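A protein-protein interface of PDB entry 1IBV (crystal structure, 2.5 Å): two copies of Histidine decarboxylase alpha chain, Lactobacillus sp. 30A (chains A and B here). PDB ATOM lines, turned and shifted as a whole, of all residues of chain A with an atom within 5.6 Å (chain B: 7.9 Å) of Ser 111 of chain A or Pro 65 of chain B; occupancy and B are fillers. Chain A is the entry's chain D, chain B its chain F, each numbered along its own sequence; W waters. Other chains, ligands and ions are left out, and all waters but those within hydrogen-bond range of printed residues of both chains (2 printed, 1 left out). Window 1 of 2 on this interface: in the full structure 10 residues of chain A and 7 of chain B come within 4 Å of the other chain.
Pro 65 of chain B touches Gly 4 of chain A (O to CA, 3.5 Å). N of Gly 4 of chain A touches CA of Gly 66 of chain B, at 3.7 Å. Gln 6 of chain A touches Ser 67 of chain B (OE1 to CA, 3.9 Å). Pro 65 of chain B touches Lys 109 of chain A (CG to O, 3.7 Å). Ser 111 of chain A touches Pro 65 of chain B (CB to CB, 3.7 Å). OG of Ser 111 of chain A touches CA of Gly 66 of chain B, at 3.7 Å.
Of the printed residues of chain B, Gly 4 of chain A touches Pro 65 (3.5 Å) and Gly 66 (3.7 Å). Ser 102 of chain A touches none of the printed residues of chain B. Ala 104 of chain A touches none of the printed residues of chain B. Pro 65 of chain B touches four residues of chain A. Of the printed residues of chain A, Gly 66 of chain B touches Gly 4 (3.7 Å) and Ser 111 (3.7 Å). The nearest residue of chain B that does not touch Ser 111 of chain A is Ser 67 of chain B (6.1 Å). The nearest residue of chain A that does not touch Pro 65 of chain B is Asp 110 of chain A (4.5 Å).
Printed residues of chain B that touch a printed residue of chain A: Pro 65, Gly 66 and Ser 67. Hydrophobic or aromatic side chains of chain B within 4 Å of the printed part of chain A: Pro 65. Along chain A the printed residues that touch a printed residue of chain B span positions 4 to 111. Among the printed residues, no Asp or Glu carboxylate lies within 4 Å of a Lys or Arg side-chain nitrogen of the other chain.
No position is printed for both chains. Of the 7 pairs that touch across the chains among the printed residues, none has its exchanged pair printed and touching as well.
Water W1 lies within hydrogen-bond range of NH2 of Arg 59 of chain B (2.7 Å) and OD1 of Asp 110 of chain A (3.1 Å). Water W2 lies within hydrogen-bond range of the side-chain hydroxyl of Tyr 62 of chain B, the backbone carbonyl oxygen of Lys 109 of chain A and the guanidinium group of Arg 59 of chain B.
The backbone carbonyl oxygen (O) of Pro 65 of chain B is in hydrogen-bond range of the backbone NH (N) of Val 5 of chain A.
O of Thr 3 of chain A sits at hydrogen-bond distance from OG of Ser 111 of chain A, 2.9 Å away. The backbone carbonyl oxygen (O) of Ala 64 of chain B sits at hydrogen-bond distance from the side-chain hydroxyl (OG) of Ser 67 of chain B. NZ of Lys 109 of chain A lies within salt-bridge range of OD2 of Asp 110 of chain A, at 3.9 Å. The backbone NH (N) of Gly 4 of chain A sits close to the side-chain hydroxyl (OG) of Ser 111 of chain A (3.4 Å).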
ATOM      1  N   PHE A   2      -0.596  19.762   8.734  1.00  0.00           N
ATOM      2  CA  PHE A   2      -1.583  20.329   7.817  1.00  0.00           C
ATOM      3  C   PHE A   2      -2.580  19.381   7.151  1.00  0.00           C
ATOM      4  O   PHE A   2      -2.374  18.176   7.067  1.00  0.00           O
ATOM      5  CB  PHE A   2      -0.866  21.125   6.717  1.00  0.00           C
ATOM      6  CG  PHE A   2       0.064  22.185   7.235  1.00  0.00           C
ATOM      7  CD1 PHE A   2      -0.327  23.519   7.276  1.00  0.00           C
ATOM      8  CD2 PHE A   2       1.327  21.841   7.712  1.00  0.00           C
ATOM      9  CE1 PHE A   2       0.520  24.488   7.785  1.00  0.00           C
ATOM     10  CE2 PHE A   2       2.175  22.801   8.220  1.00  0.00           C
ATOM     11  CZ  PHE A   2       1.773  24.127   8.257  1.00  0.00           C
ATOM     12  N   THR A   3      -3.655  19.980   6.658  1.00  0.00           N
ATOM     13  CA  THR A   3      -4.717  19.311   5.936  1.00  0.00           C
ATOM     14  C   THR A   3      -5.066  20.354   4.887  1.00  0.00           C
ATOM     15  O   THR A   3      -5.421  21.472   5.230  1.00  0.00           O
ATOM     16  CB  THR A   3      -5.928  19.001   6.841  1.00  0.00           C
ATOM     17  OG1 THR A   3      -7.036  18.584   6.036  1.00  0.00           O
ATOM     18  CG2 THR A   3      -6.330  20.204   7.655  1.00  0.00           C
ATOM     19  N   GLY A   4      -4.875  20.032   3.616  1.00  0.00           N
ATOM     20  CA  GLY A   4      -5.142  21.011   2.582  1.00  0.00           C
ATOM     21  C   GLY A   4      -6.048  20.639   1.427  1.00  0.00           C
ATOM     22  O   GLY A   4      -7.140  20.134   1.627  1.00  0.00           O
ATOM     23  N   VAL A   5      -5.563  20.866   0.212  1.00  0.00           N
ATOM     24  CA  VAL A   5      -6.328  20.600  -0.995  1.00  0.00           C
ATOM     25  C   VAL A   5      -6.908  19.198  -1.140  1.00  0.00           C
ATOM     26  O   VAL A   5      -7.793  18.984  -1.960  1.00  0.00           O
ATOM     27  CB  VAL A   5      -5.507  20.937  -2.248  1.00  0.00           C
ATOM     28  CG1 VAL A   5      -5.184  22.411  -2.267  1.00  0.00           C
ATOM     29  CG2 VAL A   5      -4.224  20.120  -2.296  1.00  0.00           C
ATOM     30  N   GLN A   6      -6.409  18.248  -0.362  1.00  0.00           N
ATOM     31  CA  GLN A   6      -6.890  16.877  -0.435  1.00  0.00           C
ATOM     32  C   GLN A   6      -7.793  16.464   0.712  1.00  0.00           C
ATOM     33  O   GLN A   6      -8.206  15.308   0.770  1.00  0.00           O
ATOM     34  CB  GLN A   6      -5.721  15.898  -0.404  1.00  0.00           C
ATOM     35  CG  GLN A   6      -4.768  15.970  -1.533  1.00  0.00           C
ATOM     36  CD  GLN A   6      -3.494  15.265  -1.198  1.00  0.00           C
ATOM     37  OE1 GLN A   6      -2.571  15.861  -0.638  1.00  0.00           O
ATOM     38  NE2 GLN A   6      -3.428  13.982  -1.512  1.00  0.00           N
ATOM     39  N   SER A 102      -7.147  25.357  11.974  1.00  0.00           N
ATOM     40  CA  SER A 102      -7.357  26.677  11.398  1.00  0.00           C
ATOM     41  C   SER A 102      -7.675  26.496   9.924  1.00  0.00           C
ATOM     42  O   SER A 102      -6.858  25.975   9.170  1.00  0.00           O
ATOM     43  CB  SER A 102      -6.101  27.528  11.577  1.00  0.00           C
ATOM     44  OG  SER A 102      -5.726  27.556  12.945  1.00  0.00           O
ATOM     45  N   ALA A 104      -8.284  27.669   6.140  1.00  0.00           N
ATOM     46  CA  ALA A 104      -7.846  28.702   5.212  1.00  0.00           C
ATOM     47  C   ALA A 104      -8.993  29.389   4.472  1.00  0.00           C
ATOM     48  O   ALA A 104      -9.988  28.753   4.137  1.00  0.00           O
ATOM     49  CB  ALA A 104      -6.865  28.105   4.223  1.00  0.00           C
ATOM     50  N   ASP A 106      -8.798  30.614   1.454  1.00  0.00           N
ATOM     51  CA  ASP A 106      -8.763  30.133   0.082  1.00  0.00           C
ATOM     52  C   ASP A 106      -8.097  28.773   0.058  1.00  0.00           C
ATOM     53  O   ASP A 106      -6.899  28.668  -0.209  1.00  0.00           O
ATOM     54  CB  ASP A 106      -7.997  31.094  -0.829  1.00  0.00           C
ATOM     55  CG  ASP A 106      -8.034  30.662  -2.286  1.00  0.00           C
ATOM     56  OD1 ASP A 106      -8.755  29.696  -2.598  1.00  0.00           O
ATOM     57  OD2 ASP A 106      -7.349  31.287  -3.122  1.00  0.00           O
ATOM     58  N   PRO A 107      -8.879  27.700   0.280  1.00  0.00           N
ATOM     59  CA  PRO A 107      -8.388  26.320   0.297  1.00  0.00           C
ATOM     60  C   PRO A 107      -7.721  25.853  -0.991  1.00  0.00           C
ATOM     61  O   PRO A 107      -7.157  24.769  -1.021  1.00  0.00           O
ATOM     62  CB  PRO A 107      -9.645  25.517   0.600  1.00  0.00           C
ATOM     63  CG  PRO A 107     -10.462  26.468   1.404  1.00  0.00           C
ATOM     64  CD  PRO A 107     -10.312  27.730   0.613  1.00  0.00           C
ATOM     65  N   LYS A 109      -5.361  27.680  -2.514  1.00  0.00           N
ATOM     66  CA  LYS A 109      -4.009  28.228  -2.509  1.00  0.00           C
ATOM     67  C   LYS A 109      -3.297  27.894  -1.216  1.00  0.00           C
ATOM     68  O   LYS A 109      -2.147  27.456  -1.227  1.00  0.00           O
ATOM     69  CB  LYS A 109      -4.016  29.751  -2.666  1.00  0.00           C
ATOM     70  CG  LYS A 109      -4.101  30.278  -4.091  1.00  0.00           C
ATOM     71  CD  LYS A 109      -3.674  31.748  -4.137  1.00  0.00           C
ATOM     72  CE  LYS A 109      -4.404  32.600  -3.066  1.00  0.00           C
ATOM     73  NZ  LYS A 109      -3.520  33.193  -1.999  1.00  0.00           N
ATOM     74  N   ASP A 110      -3.978  28.112  -0.101  1.00  0.00           N
ATOM     75  CA  ASP A 110      -3.388  27.866   1.211  1.00  0.00           C
ATOM     76  C   ASP A 110      -3.982  26.641   1.902  1.00  0.00           C
ATOM     77  O   ASP A 110      -5.172  26.351   1.753  1.00  0.00           O
ATOM     78  CB  ASP A 110      -3.580  29.102   2.110  1.00  0.00           C
ATOM     79  CG  ASP A 110      -3.056  30.380   1.474  1.00  0.00           C
ATOM     80  OD1 ASP A 110      -1.918  30.372   0.966  1.00  0.00           O
ATOM     81  OD2 ASP A 110      -3.785  31.396   1.487  1.00  0.00           O
ATOM     82  N   SER A 111      -3.155  25.919   2.651  1.00  0.00           N
ATOM     83  CA  SER A 111      -3.626  24.747   3.373  1.00  0.00           C
ATOM     84  C   SER A 111      -4.118  25.115   4.759  1.00  0.00           C
ATOM     85  O   SER A 111      -3.647  26.085   5.351  1.00  0.00           O
ATOM     86  CB  SER A 111      -2.506  23.726   3.533  1.00  0.00           C
ATOM     87  OG  SER A 111      -2.889  22.688   4.433  1.00  0.00           O
ATOM     88  N   SER A 112      -5.058  24.328   5.276  1.00  0.00           N
ATOM     89  CA  SER A 112      -5.576  24.545   6.610  1.00  0.00           C
ATOM     90  C   SER A 112      -4.474  24.013   7.503  1.00  0.00           C
ATOM     91  O   SER A 112      -3.691  23.157   7.076  1.00  0.00           O
ATOM     92  CB  SER A 112      -6.878  23.785   6.813  1.00  0.00           C
ATOM     93  OG  SER A 112      -7.895  24.329   5.989  1.00  0.00           O
ATOM     94  N   MET A 113      -4.415  24.498   8.735  1.00  0.00           N
ATOM     95  CA  MET A 113      -3.341  24.116   9.645  1.00  0.00           C
ATOM     96  C   MET A 113      -3.756  23.584  10.999  1.00  0.00           C
ATOM     97  O   MET A 113      -4.741  24.018  11.594  1.00  0.00           O
ATOM     98  CB  MET A 113      -2.418  25.326   9.832  1.00  0.00           C
ATOM     99  CG  MET A 113      -1.224  25.150  10.767  1.00  0.00           C
ATOM    100  SD  MET A 113      -0.255  26.671  10.782  1.00  0.00           S
ATOM    101  CE  MET A 113      -1.401  27.782  11.448  1.00  0.00           C
ATOM    102  N   ALA A 153      -0.590  32.743   4.843  1.00  0.00           N
ATOM    103  CA  ALA A 153      -1.794  31.943   4.735  1.00  0.00           C
ATOM    104  C   ALA A 153      -2.824  32.492   5.688  1.00  0.00           C
ATOM    105  O   ALA A 153      -2.671  32.373   6.895  1.00  0.00           O
ATOM    106  CB  ALA A 153      -1.489  30.517   5.082  1.00  0.00           C
ATOM    107  N   PHE A 155      -6.409  32.559   7.515  1.00  0.00           N
ATOM    108  CA  PHE A 155      -7.435  31.635   7.955  1.00  0.00           C
ATOM    109  C   PHE A 155      -8.712  32.410   8.229  1.00  0.00           C
ATOM    110  O   PHE A 155      -8.687  33.625   8.405  1.00  0.00           O
ATOM    111  CB  PHE A 155      -6.973  30.906   9.216  1.00  0.00           C
ATOM    112  CG  PHE A 155      -5.587  30.338   9.102  1.00  0.00           C
ATOM    113  CD1 PHE A 155      -5.333  29.272   8.252  1.00  0.00           C
ATOM    114  CD2 PHE A 155      -4.523  30.902   9.800  1.00  0.00           C
ATOM    115  CE1 PHE A 155      -4.040  28.783   8.090  1.00  0.00           C
ATOM    116  CE2 PHE A 155      -3.222  30.418   9.639  1.00  0.00           C
ATOM    117  CZ  PHE A 155      -2.985  29.355   8.786  1.00  0.00           C
ATOM    118  N   ARG B  59       7.582  31.389  -5.264  1.00  0.00           N
ATOM    119  CA  ARG B  59       7.229  29.972  -5.280  1.00  0.00           C
ATOM    120  C   ARG B  59       7.201  29.325  -6.653  1.00  0.00           C
ATOM    121  O   ARG B  59       6.646  29.870  -7.610  1.00  0.00           O
ATOM    122  CB  ARG B  59       5.883  29.762  -4.595  1.00  0.00           C
ATOM    123  CG  ARG B  59       5.844  30.243  -3.167  1.00  0.00           C
ATOM    124  CD  ARG B  59       4.520  29.935  -2.534  1.00  0.00           C
ATOM    125  NE  ARG B  59       4.409  30.559  -1.228  1.00  0.00           N
ATOM    126  CZ  ARG B  59       3.454  30.285  -0.354  1.00  0.00           C
ATOM    127  NH1 ARG B  59       3.419  30.903   0.818  1.00  0.00           N
ATOM    128  NH2 ARG B  59       2.546  29.370  -0.642  1.00  0.00           N
ATOM    129  N   TYR B  62       7.012  23.802  -5.347  1.00  0.00           N
ATOM    130  CA  TYR B  62       7.044  23.377  -3.962  1.00  0.00           C
ATOM    131  C   TYR B  62       5.994  22.304  -3.748  1.00  0.00           C
ATOM    132  O   TYR B  62       5.090  22.138  -4.560  1.00  0.00           O
ATOM    133  CB  TYR B  62       6.790  24.575  -3.047  1.00  0.00           C
ATOM    134  CG  TYR B  62       5.415  25.178  -3.165  1.00  0.00           C
ATOM    135  CD1 TYR B  62       5.104  26.049  -4.205  1.00  0.00           C
ATOM    136  CD2 TYR B  62       4.433  24.900  -2.216  1.00  0.00           C
ATOM    137  CE1 TYR B  62       3.852  26.629  -4.292  1.00  0.00           C
ATOM    138  CE2 TYR B  62       3.183  25.474  -2.292  1.00  0.00           C
ATOM    139  CZ  TYR B  62       2.898  26.337  -3.330  1.00  0.00           C
ATOM    140  OH  TYR B  62       1.656  26.912  -3.407  1.00  0.00           O
ATOM    141  N   PRO B  63       6.089  21.561  -2.639  1.00  0.00           N
ATOM    142  CA  PRO B  63       5.136  20.500  -2.325  1.00  0.00           C
ATOM    143  C   PRO B  63       3.720  21.019  -2.203  1.00  0.00           C
ATOM    144  O   PRO B  63       3.503  22.159  -1.793  1.00  0.00           O
ATOM    145  CB  PRO B  63       5.655  19.966  -1.002  1.00  0.00           C
ATOM    146  CG  PRO B  63       7.109  20.201  -1.104  1.00  0.00           C
ATOM    147  CD  PRO B  63       7.160  21.595  -1.636  1.00  0.00           C
ATOM    148  N   ALA B  64       2.764  20.172  -2.560  1.00  0.00           N
ATOM    149  CA  ALA B  64       1.361  20.530  -2.506  1.00  0.00           C
ATOM    150  C   ALA B  64       0.910  20.866  -1.081  1.00  0.00           C
ATOM    151  O   ALA B  64       1.352  20.245  -0.112  1.00  0.00           O
ATOM    152  CB  ALA B  64       0.515  19.389  -3.091  1.00  0.00           C
ATOM    153  N   PRO B  65       0.043  21.876  -0.933  1.00  0.00           N
ATOM    154  CA  PRO B  65      -0.472  22.304   0.365  1.00  0.00           C
ATOM    155  C   PRO B  65      -1.197  21.182   1.083  1.00  0.00           C
ATOM    156  O   PRO B  65      -2.263  20.743   0.643  1.00  0.00           O
ATOM    157  CB  PRO B  65      -1.440  23.419  -0.009  1.00  0.00           C
ATOM    158  CG  PRO B  65      -0.812  24.000  -1.220  1.00  0.00           C
ATOM    159  CD  PRO B  65      -0.420  22.780  -1.996  1.00  0.00           C
ATOM    160  N   GLY B  66      -0.615  20.735   2.187  1.00  0.00           N
ATOM    161  CA  GLY B  66      -1.207  19.678   2.979  1.00  0.00           C
ATOM    162  C   GLY B  66      -0.737  18.292   2.588  1.00  0.00           C
ATOM    163  O   GLY B  66      -1.190  17.301   3.152  1.00  0.00           O
ATOM    164  N   SER B  67       0.158  18.220   1.613  1.00  0.00           N
ATOM    165  CA  SER B  67       0.663  16.943   1.154  1.00  0.00           C
ATOM    166  C   SER B  67       1.461  16.267   2.238  1.00  0.00           C
ATOM    167  O   SER B  67       1.837  16.894   3.222  1.00  0.00           O
ATOM    168  CB  SER B  67       1.540  17.129  -0.081  1.00  0.00           C
ATOM    169  OG  SER B  67       2.650  17.960   0.188  1.00  0.00           O
ATOM    170  N   PHE B  68       1.698  14.975   2.071  1.00  0.00           N
ATOM    171  CA  PHE B  68       2.471  14.219   3.028  1.00  0.00           C
ATOM    172  C   PHE B  68       3.789  13.937   2.352  1.00  0.00           C
ATOM    173  O   PHE B  68       3.839  13.272   1.330  1.00  0.00           O
ATOM    174  CB  PHE B  68       1.753  12.927   3.411  1.00  0.00           C
ATOM    175  CG  PHE B  68       0.705  13.120   4.470  1.00  0.00           C
ATOM    176  CD1 PHE B  68      -0.455  13.822   4.192  1.00  0.00           C
ATOM    177  CD2 PHE B  68       0.903  12.646   5.759  1.00  0.00           C
ATOM    178  CE1 PHE B  68      -1.394  14.059   5.178  1.00  0.00           C
ATOM    179  CE2 PHE B  68      -0.034  12.879   6.748  1.00  0.00           C
ATOM    180  CZ  PHE B  68      -1.183  13.587   6.456  1.00  0.00           C
HETATM  181  O   HOH W   1       1.019  29.497   1.640  1.00  0.00           O
HETATM  182  O   HOH W   2       0.613  26.983  -0.803  1.00  0.00           O
